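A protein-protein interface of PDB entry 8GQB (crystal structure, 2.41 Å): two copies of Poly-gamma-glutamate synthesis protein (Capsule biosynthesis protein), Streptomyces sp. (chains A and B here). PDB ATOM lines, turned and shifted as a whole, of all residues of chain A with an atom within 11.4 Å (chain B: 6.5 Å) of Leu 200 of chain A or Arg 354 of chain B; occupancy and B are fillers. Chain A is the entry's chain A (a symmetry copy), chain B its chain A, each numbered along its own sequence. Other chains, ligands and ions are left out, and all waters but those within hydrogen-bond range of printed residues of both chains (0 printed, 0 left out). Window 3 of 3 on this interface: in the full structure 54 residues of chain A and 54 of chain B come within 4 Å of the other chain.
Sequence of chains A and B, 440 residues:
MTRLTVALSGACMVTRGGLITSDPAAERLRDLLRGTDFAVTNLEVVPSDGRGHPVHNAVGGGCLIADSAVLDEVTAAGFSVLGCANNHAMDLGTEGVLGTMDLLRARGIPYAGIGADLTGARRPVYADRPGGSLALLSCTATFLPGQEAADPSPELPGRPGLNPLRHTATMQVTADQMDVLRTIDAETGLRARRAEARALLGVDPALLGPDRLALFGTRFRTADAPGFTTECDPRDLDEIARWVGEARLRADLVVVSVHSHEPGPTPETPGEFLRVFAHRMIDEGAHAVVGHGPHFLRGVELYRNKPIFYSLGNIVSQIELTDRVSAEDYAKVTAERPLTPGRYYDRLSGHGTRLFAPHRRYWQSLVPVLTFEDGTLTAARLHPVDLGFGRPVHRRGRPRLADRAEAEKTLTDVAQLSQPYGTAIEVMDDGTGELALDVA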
ATOM      1  N   ALA A 192      -2.961  -4.837  30.890  1.00  0.00           N
ATOM      2  CA  ALA A 192      -3.592  -5.838  30.035  1.00  0.00           C
ATOM      3  C   ALA A 192      -4.445  -5.191  28.951  1.00  0.00           C
ATOM      4  O   ALA A 192      -4.447  -5.644  27.801  1.00  0.00           O
ATOM      5  CB  ALA A 192      -4.440  -6.790  30.877  1.00  0.00           C
ATOM      6  N   ARG A 193      -5.169  -4.125  29.296  1.00  0.00           N
ATOM      7  CA  ARG A 193      -6.044  -3.452  28.341  1.00  0.00           C
ATOM      8  C   ARG A 193      -5.289  -2.695  27.257  1.00  0.00           C
ATOM      9  O   ARG A 193      -5.936  -2.145  26.359  1.00  0.00           O
ATOM     10  CB  ARG A 193      -6.989  -2.508  29.084  1.00  0.00           C
ATOM     11  CG  ARG A 193      -8.217  -3.221  29.609  1.00  0.00           C
ATOM     12  CD  ARG A 193      -8.851  -2.509  30.781  1.00  0.00           C
ATOM     13  NE  ARG A 193     -10.026  -3.232  31.259  1.00  0.00           N
ATOM     14  CZ  ARG A 193      -9.975  -4.285  32.068  1.00  0.00           C
ATOM     15  NH1 ARG A 193     -11.096  -4.880  32.455  1.00  0.00           N
ATOM     16  NH2 ARG A 193      -8.804  -4.745  32.491  1.00  0.00           N
ATOM     17  N   ARG A 194      -3.959  -2.646  27.303  1.00  0.00           N
ATOM     18  CA  ARG A 194      -3.177  -2.113  26.196  1.00  0.00           C
ATOM     19  C   ARG A 194      -2.670  -3.209  25.270  1.00  0.00           C
ATOM     20  O   ARG A 194      -1.961  -2.909  24.302  1.00  0.00           O
ATOM     21  CB  ARG A 194      -2.007  -1.277  26.721  1.00  0.00           C
ATOM     22  CG  ARG A 194      -2.440  -0.071  27.534  1.00  0.00           C
ATOM     23  CD  ARG A 194      -1.305   0.921  27.748  1.00  0.00           C
ATOM     24  NE  ARG A 194      -0.165   0.315  28.427  1.00  0.00           N
ATOM     25  CZ  ARG A 194      -0.012   0.277  29.746  1.00  0.00           C
ATOM     26  NH1 ARG A 194      -0.930   0.814  30.540  1.00  0.00           N
ATOM     27  NH2 ARG A 194       1.060  -0.300  30.272  1.00  0.00           N
ATOM     28  N   ALA A 195      -3.044  -4.468  25.537  1.00  0.00           N
ATOM     29  CA  ALA A 195      -2.511  -5.608  24.793  1.00  0.00           C
ATOM     30  C   ALA A 195      -2.641  -5.417  23.287  1.00  0.00           C
ATOM     31  O   ALA A 195      -1.669  -5.592  22.544  1.00  0.00           O
ATOM     32  CB  ALA A 195      -3.214  -6.894  25.230  1.00  0.00           C
ATOM     33  N   GLU A 196      -3.840  -5.057  22.817  1.00  0.00           N
ATOM     34  CA  GLU A 196      -4.017  -4.813  21.389  1.00  0.00           C
ATOM     35  C   GLU A 196      -3.082  -3.710  20.908  1.00  0.00           C
ATOM     36  O   GLU A 196      -2.348  -3.891  19.928  1.00  0.00           O
ATOM     37  CB  GLU A 196      -5.472  -4.459  21.077  1.00  0.00           C
ATOM     38  CG  GLU A 196      -5.800  -4.543  19.587  1.00  0.00           C
ATOM     39  CD  GLU A 196      -7.127  -3.898  19.236  1.00  0.00           C
ATOM     40  OE1 GLU A 196      -7.844  -3.476  20.168  1.00  0.00           O
ATOM     41  OE2 GLU A 196      -7.451  -3.805  18.031  1.00  0.00           O
ATOM     42  N   ALA A 197      -3.072  -2.568  21.603  1.00  0.00           N
ATOM     43  CA  ALA A 197      -2.150  -1.491  21.254  1.00  0.00           C
ATOM     44  C   ALA A 197      -0.697  -1.945  21.301  1.00  0.00           C
ATOM     45  O   ALA A 197       0.157  -1.328  20.656  1.00  0.00           O
ATOM     46  CB  ALA A 197      -2.354  -0.293  22.181  1.00  0.00           C
ATOM     47  N   ARG A 198      -0.404  -3.019  22.038  1.00  0.00           N
ATOM     48  CA  ARG A 198       0.938  -3.590  22.031  1.00  0.00           C
ATOM     49  C   ARG A 198       1.236  -4.276  20.702  1.00  0.00           C
ATOM     50  O   ARG A 198       2.302  -4.070  20.109  1.00  0.00           O
ATOM     51  CB  ARG A 198       1.084  -4.579  23.184  1.00  0.00           C
ATOM     52  CG  ARG A 198       2.486  -4.699  23.743  1.00  0.00           C
ATOM     53  CD  ARG A 198       2.472  -4.373  25.223  1.00  0.00           C
ATOM     54  NE  ARG A 198       1.412  -5.099  25.915  1.00  0.00           N
ATOM     55  CZ  ARG A 198       0.872  -4.716  27.066  1.00  0.00           C
ATOM     56  NH1 ARG A 198      -0.089  -5.440  27.623  1.00  0.00           N
ATOM     57  NH2 ARG A 198       1.287  -3.604  27.658  1.00  0.00           N
ATOM     58  N   ALA A 199       0.303  -5.099  20.215  1.00  0.00           N
ATOM     59  CA  ALA A 199       0.556  -5.872  19.003  1.00  0.00           C
ATOM     60  C   ALA A 199       0.453  -5.022  17.742  1.00  0.00           C
ATOM     61  O   ALA A 199       1.097  -5.335  16.735  1.00  0.00           O
ATOM     62  CB  ALA A 199      -0.409  -7.055  18.921  1.00  0.00           C
ATOM     63  N   LEU A 200      -0.338  -3.949  17.778  1.00  0.00           N
ATOM     64  CA  LEU A 200      -0.490  -3.088  16.610  1.00  0.00           C
ATOM     65  C   LEU A 200       0.664  -2.099  16.490  1.00  0.00           C
ATOM     66  O   LEU A 200       1.223  -1.915  15.403  1.00  0.00           O
ATOM     67  CB  LEU A 200      -1.830  -2.352  16.675  1.00  0.00           C
ATOM     68  CG  LEU A 200      -3.073  -3.225  16.491  1.00  0.00           C
ATOM     69  CD1 LEU A 200      -4.329  -2.485  16.919  1.00  0.00           C
ATOM     70  CD2 LEU A 200      -3.186  -3.679  15.044  1.00  0.00           C
ATOM     71  N   LEU A 201       1.036  -1.453  17.598  1.00  0.00           N
ATOM     72  CA  LEU A 201       2.156  -0.521  17.579  1.00  0.00           C
ATOM     73  C   LEU A 201       3.508  -1.222  17.615  1.00  0.00           C
ATOM     74  O   LEU A 201       4.512  -0.622  17.218  1.00  0.00           O
ATOM     75  CB  LEU A 201       2.066   0.451  18.758  1.00  0.00           C
ATOM     76  CG  LEU A 201       0.899   1.440  18.777  1.00  0.00           C
ATOM     77  CD1 LEU A 201       1.034   2.404  19.949  1.00  0.00           C
ATOM     78  CD2 LEU A 201       0.812   2.199  17.463  1.00  0.00           C
ATOM     79  N   GLY A 202       3.557  -2.471  18.078  1.00  0.00           N
ATOM     80  CA  GLY A 202       4.798  -3.190  18.240  1.00  0.00           C
ATOM     81  C   GLY A 202       5.426  -3.067  19.613  1.00  0.00           C
ATOM     82  O   GLY A 202       6.194  -3.950  20.010  1.00  0.00           O
ATOM     83  N   VAL A 203       5.119  -1.998  20.351  1.00  0.00           N
ATOM     84  CA  VAL A 203       5.646  -1.790  21.694  1.00  0.00           C
ATOM     85  C   VAL A 203       4.586  -1.068  22.515  1.00  0.00           C
ATOM     86  O   VAL A 203       3.646  -0.478  21.976  1.00  0.00           O
ATOM     87  CB  VAL A 203       6.976  -0.995  21.681  1.00  0.00           C
ATOM     88  CG1 VAL A 203       6.710   0.500  21.564  1.00  0.00           C
ATOM     89  CG2 VAL A 203       7.814  -1.315  22.914  1.00  0.00           C
ATOM     90  N   ASP A 204       4.738  -1.125  23.830  1.00  0.00           N
ATOM     91  CA  ASP A 204       3.788  -0.489  24.734  1.00  0.00           C
ATOM     92  C   ASP A 204       3.910   1.027  24.631  1.00  0.00           C
ATOM     93  O   ASP A 204       5.005   1.565  24.845  1.00  0.00           O
ATOM     94  CB  ASP A 204       4.042  -0.951  26.167  1.00  0.00           C
ATOM     95  CG  ASP A 204       2.857  -0.702  27.087  1.00  0.00           C
ATOM     96  OD1 ASP A 204       2.120   0.285  26.877  1.00  0.00           O
ATOM     97  OD2 ASP A 204       2.662  -1.500  28.028  1.00  0.00           O
ATOM     98  N   PRO A 205       2.832   1.752  24.315  1.00  0.00           N
ATOM     99  CA  PRO A 205       2.912   3.220  24.274  1.00  0.00           C
ATOM    100  C   PRO A 205       3.120   3.867  25.634  1.00  0.00           C
ATOM    101  O   PRO A 205       3.285   5.092  25.697  1.00  0.00           O
ATOM    102  CB  PRO A 205       1.557   3.626  23.672  1.00  0.00           C
ATOM    103  CG  PRO A 205       0.647   2.491  23.995  1.00  0.00           C
ATOM    104  CD  PRO A 205       1.501   1.259  23.918  1.00  0.00           C
ATOM    105  N   GLU B 320      -7.178   2.952   4.287  1.00  0.00           N
ATOM    106  CA  GLU B 320      -5.961   3.336   3.583  1.00  0.00           C
ATOM    107  C   GLU B 320      -6.219   3.825   2.164  1.00  0.00           C
ATOM    108  O   GLU B 320      -5.273   4.261   1.498  1.00  0.00           O
ATOM    109  CB  GLU B 320      -4.983   2.160   3.553  1.00  0.00           C
ATOM    110  CG  GLU B 320      -4.428   1.776   4.915  1.00  0.00           C
ATOM    111  CD  GLU B 320      -3.611   0.497   4.872  1.00  0.00           C
ATOM    112  OE1 GLU B 320      -4.177  -0.561   4.525  1.00  0.00           O
ATOM    113  OE2 GLU B 320      -2.401   0.552   5.177  1.00  0.00           O
ATOM    114  N   LEU B 348       2.608   5.075   7.159  1.00  0.00           N
ATOM    115  CA  LEU B 348       1.932   5.044   8.452  1.00  0.00           C
ATOM    116  C   LEU B 348       1.926   3.645   9.053  1.00  0.00           C
ATOM    117  O   LEU B 348       1.941   3.498  10.280  1.00  0.00           O
ATOM    118  CB  LEU B 348       0.503   5.569   8.300  1.00  0.00           C
ATOM    119  CG  LEU B 348      -0.373   5.682   9.551  1.00  0.00           C
ATOM    120  CD1 LEU B 348       0.277   6.591  10.581  1.00  0.00           C
ATOM    121  CD2 LEU B 348      -1.760   6.188   9.183  1.00  0.00           C
ATOM    122  N   SER B 349       1.907   2.610   8.214  1.00  0.00           N
ATOM    123  CA  SER B 349       1.928   1.227   8.669  1.00  0.00           C
ATOM    124  C   SER B 349       3.294   0.576   8.482  1.00  0.00           C
ATOM    125  O   SER B 349       3.402  -0.653   8.551  1.00  0.00           O
ATOM    126  CB  SER B 349       0.855   0.416   7.941  1.00  0.00           C
ATOM    127  OG  SER B 349       1.098   0.388   6.545  1.00  0.00           O
ATOM    128  N   GLY B 350       4.335   1.370   8.252  1.00  0.00           N
ATOM    129  CA  GLY B 350       5.645   0.809   7.961  1.00  0.00           C
ATOM    130  C   GLY B 350       5.661  -0.016   6.693  1.00  0.00           C
ATOM    131  O   GLY B 350       6.356  -1.038   6.626  1.00  0.00           O
ATOM    132  N   HIS B 351       4.907   0.412   5.683  1.00  0.00           N
ATOM    133  CA  HIS B 351       4.694  -0.341   4.448  1.00  0.00           C
ATOM    134  C   HIS B 351       4.184  -1.751   4.752  1.00  0.00           C
ATOM    135  O   HIS B 351       4.774  -2.761   4.364  1.00  0.00           O
ATOM    136  CB  HIS B 351       5.961  -0.379   3.588  1.00  0.00           C
ATOM    137  CG  HIS B 351       5.704  -0.723   2.153  1.00  0.00           C
ATOM    138  ND1 HIS B 351       4.527  -1.300   1.726  1.00  0.00           N
ATOM    139  CD2 HIS B 351       6.466  -0.559   1.045  1.00  0.00           C
ATOM    140  CE1 HIS B 351       4.578  -1.485   0.419  1.00  0.00           C
ATOM    141  NE2 HIS B 351       5.743  -1.043  -0.018  1.00  0.00           N
ATOM    142  N   GLY B 352       3.064  -1.797   5.471  1.00  0.00           N
ATOM    143  CA  GLY B 352       2.349  -3.031   5.715  1.00  0.00           C
ATOM    144  C   GLY B 352       2.908  -3.923   6.801  1.00  0.00           C
ATOM    145  O   GLY B 352       2.378  -5.023   7.003  1.00  0.00           O
ATOM    146  N   THR B 353       3.954  -3.499   7.509  1.00  0.00           N
ATOM    147  CA  THR B 353       4.539  -4.319   8.562  1.00  0.00           C
ATOM    148  C   THR B 353       3.915  -4.076   9.929  1.00  0.00           C
ATOM    149  O   THR B 353       4.211  -4.824  10.868  1.00  0.00           O
ATOM    150  CB  THR B 353       6.050  -4.077   8.653  1.00  0.00           C
ATOM    151  OG1 THR B 353       6.298  -2.737   9.097  1.00  0.00           O
ATOM    152  CG2 THR B 353       6.707  -4.288   7.297  1.00  0.00           C
ATOM    153  N   ARG B 354       3.065  -3.063  10.068  1.00  0.00           N
ATOM    154  CA  ARG B 354       2.440  -2.729  11.338  1.00  0.00           C
ATOM    155  C   ARG B 354       0.942  -2.534  11.130  1.00  0.00           C
ATOM    156  O   ARG B 354       0.421  -2.675  10.019  1.00  0.00           O
ATOM    157  CB  ARG B 354       3.075  -1.475  11.955  1.00  0.00           C
ATOM    158  N   LEU B 355       0.256  -2.216  12.222  1.00  0.00           N
ATOM    159  CA  LEU B 355      -1.182  -1.914  12.234  1.00  0.00           C
ATOM    160  C   LEU B 355      -1.956  -3.169  11.807  1.00  0.00           C
ATOM    161  O   LEU B 355      -1.529  -4.298  12.082  1.00  0.00           O
ATOM    162  CB  LEU B 355      -1.450  -0.672  11.400  1.00  0.00           C
ATOM    163  CG  LEU B 355      -0.721   0.580  11.902  1.00  0.00           C
ATOM    164  CD1 LEU B 355      -1.017   1.788  11.024  1.00  0.00           C
ATOM    165  CD2 LEU B 355      -1.080   0.867  13.354  1.00  0.00           C
ATOM    166  N   PHE B 356      -3.094  -2.987  11.134  1.00  0.00           N
ATOM    167  CA  PHE B 356      -4.051  -4.074  10.954  1.00  0.00           C
ATOM    168  C   PHE B 356      -3.725  -4.992   9.782  1.00  0.00           C
ATOM    169  O   PHE B 356      -4.292  -6.087   9.699  1.00  0.00           O
ATOM    170  CB  PHE B 356      -5.459  -3.500  10.772  1.00  0.00           C
ATOM    171  CG  PHE B 356      -5.859  -2.533  11.849  1.00  0.00           C
ATOM    172  CD1 PHE B 356      -6.200  -2.985  13.110  1.00  0.00           C
ATOM    173  CD2 PHE B 356      -5.894  -1.170  11.598  1.00  0.00           C
ATOM    174  CE1 PHE B 356      -6.569  -2.099  14.106  1.00  0.00           C
ATOM    175  CE2 PHE B 356      -6.262  -0.277  12.590  1.00  0.00           C
ATOM    176  CZ  PHE B 356      -6.597  -0.743  13.846  1.00  0.00           C
ATOM    177  N   ALA B 357      -2.830  -4.583   8.885  1.00  0.00           N
ATOM    178  CA  ALA B 357      -2.581  -5.365   7.674  1.00  0.00           C
ATOM    179  C   ALA B 357      -2.007  -6.756   7.939  1.00  0.00           C
ATOM    180  O   ALA B 357      -2.509  -7.724   7.342  1.00  0.00           O
ATOM    181  CB  ALA B 357      -1.679  -4.566   6.729  1.00  0.00           C
ATOM    182  N   PRO B 358      -0.981  -6.942   8.783  1.00  0.00           N
ATOM    183  CA  PRO B 358      -0.310  -8.254   8.833  1.00  0.00           C
ATOM    184  C   PRO B 358      -1.128  -9.381   9.455  1.00  0.00           C
ATOM    185  O   PRO B 358      -0.731 -10.545   9.307  1.00  0.00           O
ATOM    186  CB  PRO B 358       0.948  -7.976   9.673  1.00  0.00           C
ATOM    187  CG  PRO B 358       1.115  -6.495   9.653  1.00  0.00           C
ATOM    188  CD  PRO B 358      -0.270  -5.953   9.612  1.00  0.00           C
ATOM    189  N   HIS B 359      -2.236  -9.100  10.134  1.00  0.00           N
ATOM    190  CA  HIS B 359      -2.943 -10.112  10.910  1.00  0.00           C
ATOM    191  C   HIS B 359      -4.292 -10.440  10.281  1.00  0.00           C
ATOM    192  O   HIS B 359      -4.978  -9.558   9.755  1.00  0.00           O
ATOM    193  CB  HIS B 359      -3.119  -9.650  12.357  1.00  0.00           C
ATOM    194  CG  HIS B 359      -1.828  -9.307  13.033  1.00  0.00           C
ATOM    195  ND1 HIS B 359      -1.445  -8.009  13.297  1.00  0.00           N
ATOM    196  CD2 HIS B 359      -0.816 -10.094  13.472  1.00  0.00           C
ATOM    197  CE1 HIS B 359      -0.262  -8.013  13.884  1.00  0.00           C
ATOM    198  NE2 HIS B 359       0.143  -9.265  14.002  1.00  0.00           N
ATOM    199  N   TYR B 362      -8.249  -9.344  11.390  1.00  0.00           N
ATOM    200  CA  TYR B 362      -8.716  -8.019  11.006  1.00  0.00           C
ATOM    201  C   TYR B 362      -9.371  -7.985   9.631  1.00  0.00           C
ATOM    202  O   TYR B 362      -9.851  -6.924   9.221  1.00  0.00           O
ATOM    203  CB  TYR B 362      -7.557  -7.017  11.035  1.00  0.00           C
ATOM    204  CG  TYR B 362      -7.015  -6.734  12.416  1.00  0.00           C
ATOM    205  CD1 TYR B 362      -7.793  -6.087  13.366  1.00  0.00           C
ATOM    206  CD2 TYR B 362      -5.723  -7.097  12.765  1.00  0.00           C
ATOM    207  CE1 TYR B 362      -7.304  -5.820  14.631  1.00  0.00           C
ATOM    208  CE2 TYR B 362      -5.222  -6.831  14.027  1.00  0.00           C
ATOM    209  CZ  TYR B 362      -6.017  -6.192  14.955  1.00  0.00           C
ATOM    210  OH  TYR B 362      -5.527  -5.923  16.213  1.00  0.00           O
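The backbone carbonyl oxygen (O) of Leu 200 of chain A is in hydrogen-bond range of the backbone NH (N) of Leu 355 of chain B (3.3 Å). OH of Tyr 362 of chain B sits at hydrogen-bond distance from OE2 of Glu 196 of chain A (3.4 Å).
The backbone carbonyl oxygen of Ser 349 of chain B sits at hydrogen-bond distance from the backbone NH of Arg 354 of chain B (2.9 Å).
Arg 354 of chain B touches Leu 200 of chain A. Phe 356 of chain B touches Leu 200 of chain A. Tyr 362 of chain B touches Leu 200 of chain A (OH to CD2, 3.4 Å).
Of the printed residues of chain B, Glu 196 of chain A touches Tyr 362. Leu 200 of chain A touches just these residues of chain B: Arg 354 (3.9 Å), Leu 355 (3.3 Å), Phe 356 (3.6 Å) and Tyr 362 (3.4 Å). Asp 204 of chain A touches none of the printed residues of chain B. No residue of chain A comes within 4 Å of Ser 349 of chain B. Gly 350 of chain B touches none of the printed residues of chain A. No residue of chain A comes within 4 Å of Gly 352 of chain B. No residue of chain A comes within 4 Å of Thr 353 of chain B. Arg 354 of chain B touches just one residue of chain A: Leu 200. Of chain A, only Leu 200 comes within 4 Å of Phe 356 of chain B. Of the printed residues of chain A, Tyr 362 of chain B touches Glu 196 (3.4 Å) and Leu 200 (3.4 Å). The nearest residue of chain A that does not touch Arg 354 of chain B is Leu 201 of chain A (5.5 Å). The nearest printed residue of chain B that does not touch Glu 196 of chain A is Phe 356 of chain B (4.4 Å).
Of the 14 printed residues of chain A, 2 touch a printed residue of chain B. Printed residues of chain A that touch a printed residue of chain B: Glu 196 and Leu 200. Of the 14 printed residues of chain B, 4 touch a printed residue of chain A. Along chain B the printed residues that touch a printed residue of chain A span positions 354 to 362. Among the printed residues, no Asp or Glu carboxylate lies within 4 Å of a Lys or Arg side-chain nitrogen of the other chain.
No position is printed for both chains. Of the 5 pairs that touch across the chains among the printed residues, none has its exchanged pair printed and touching as well.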
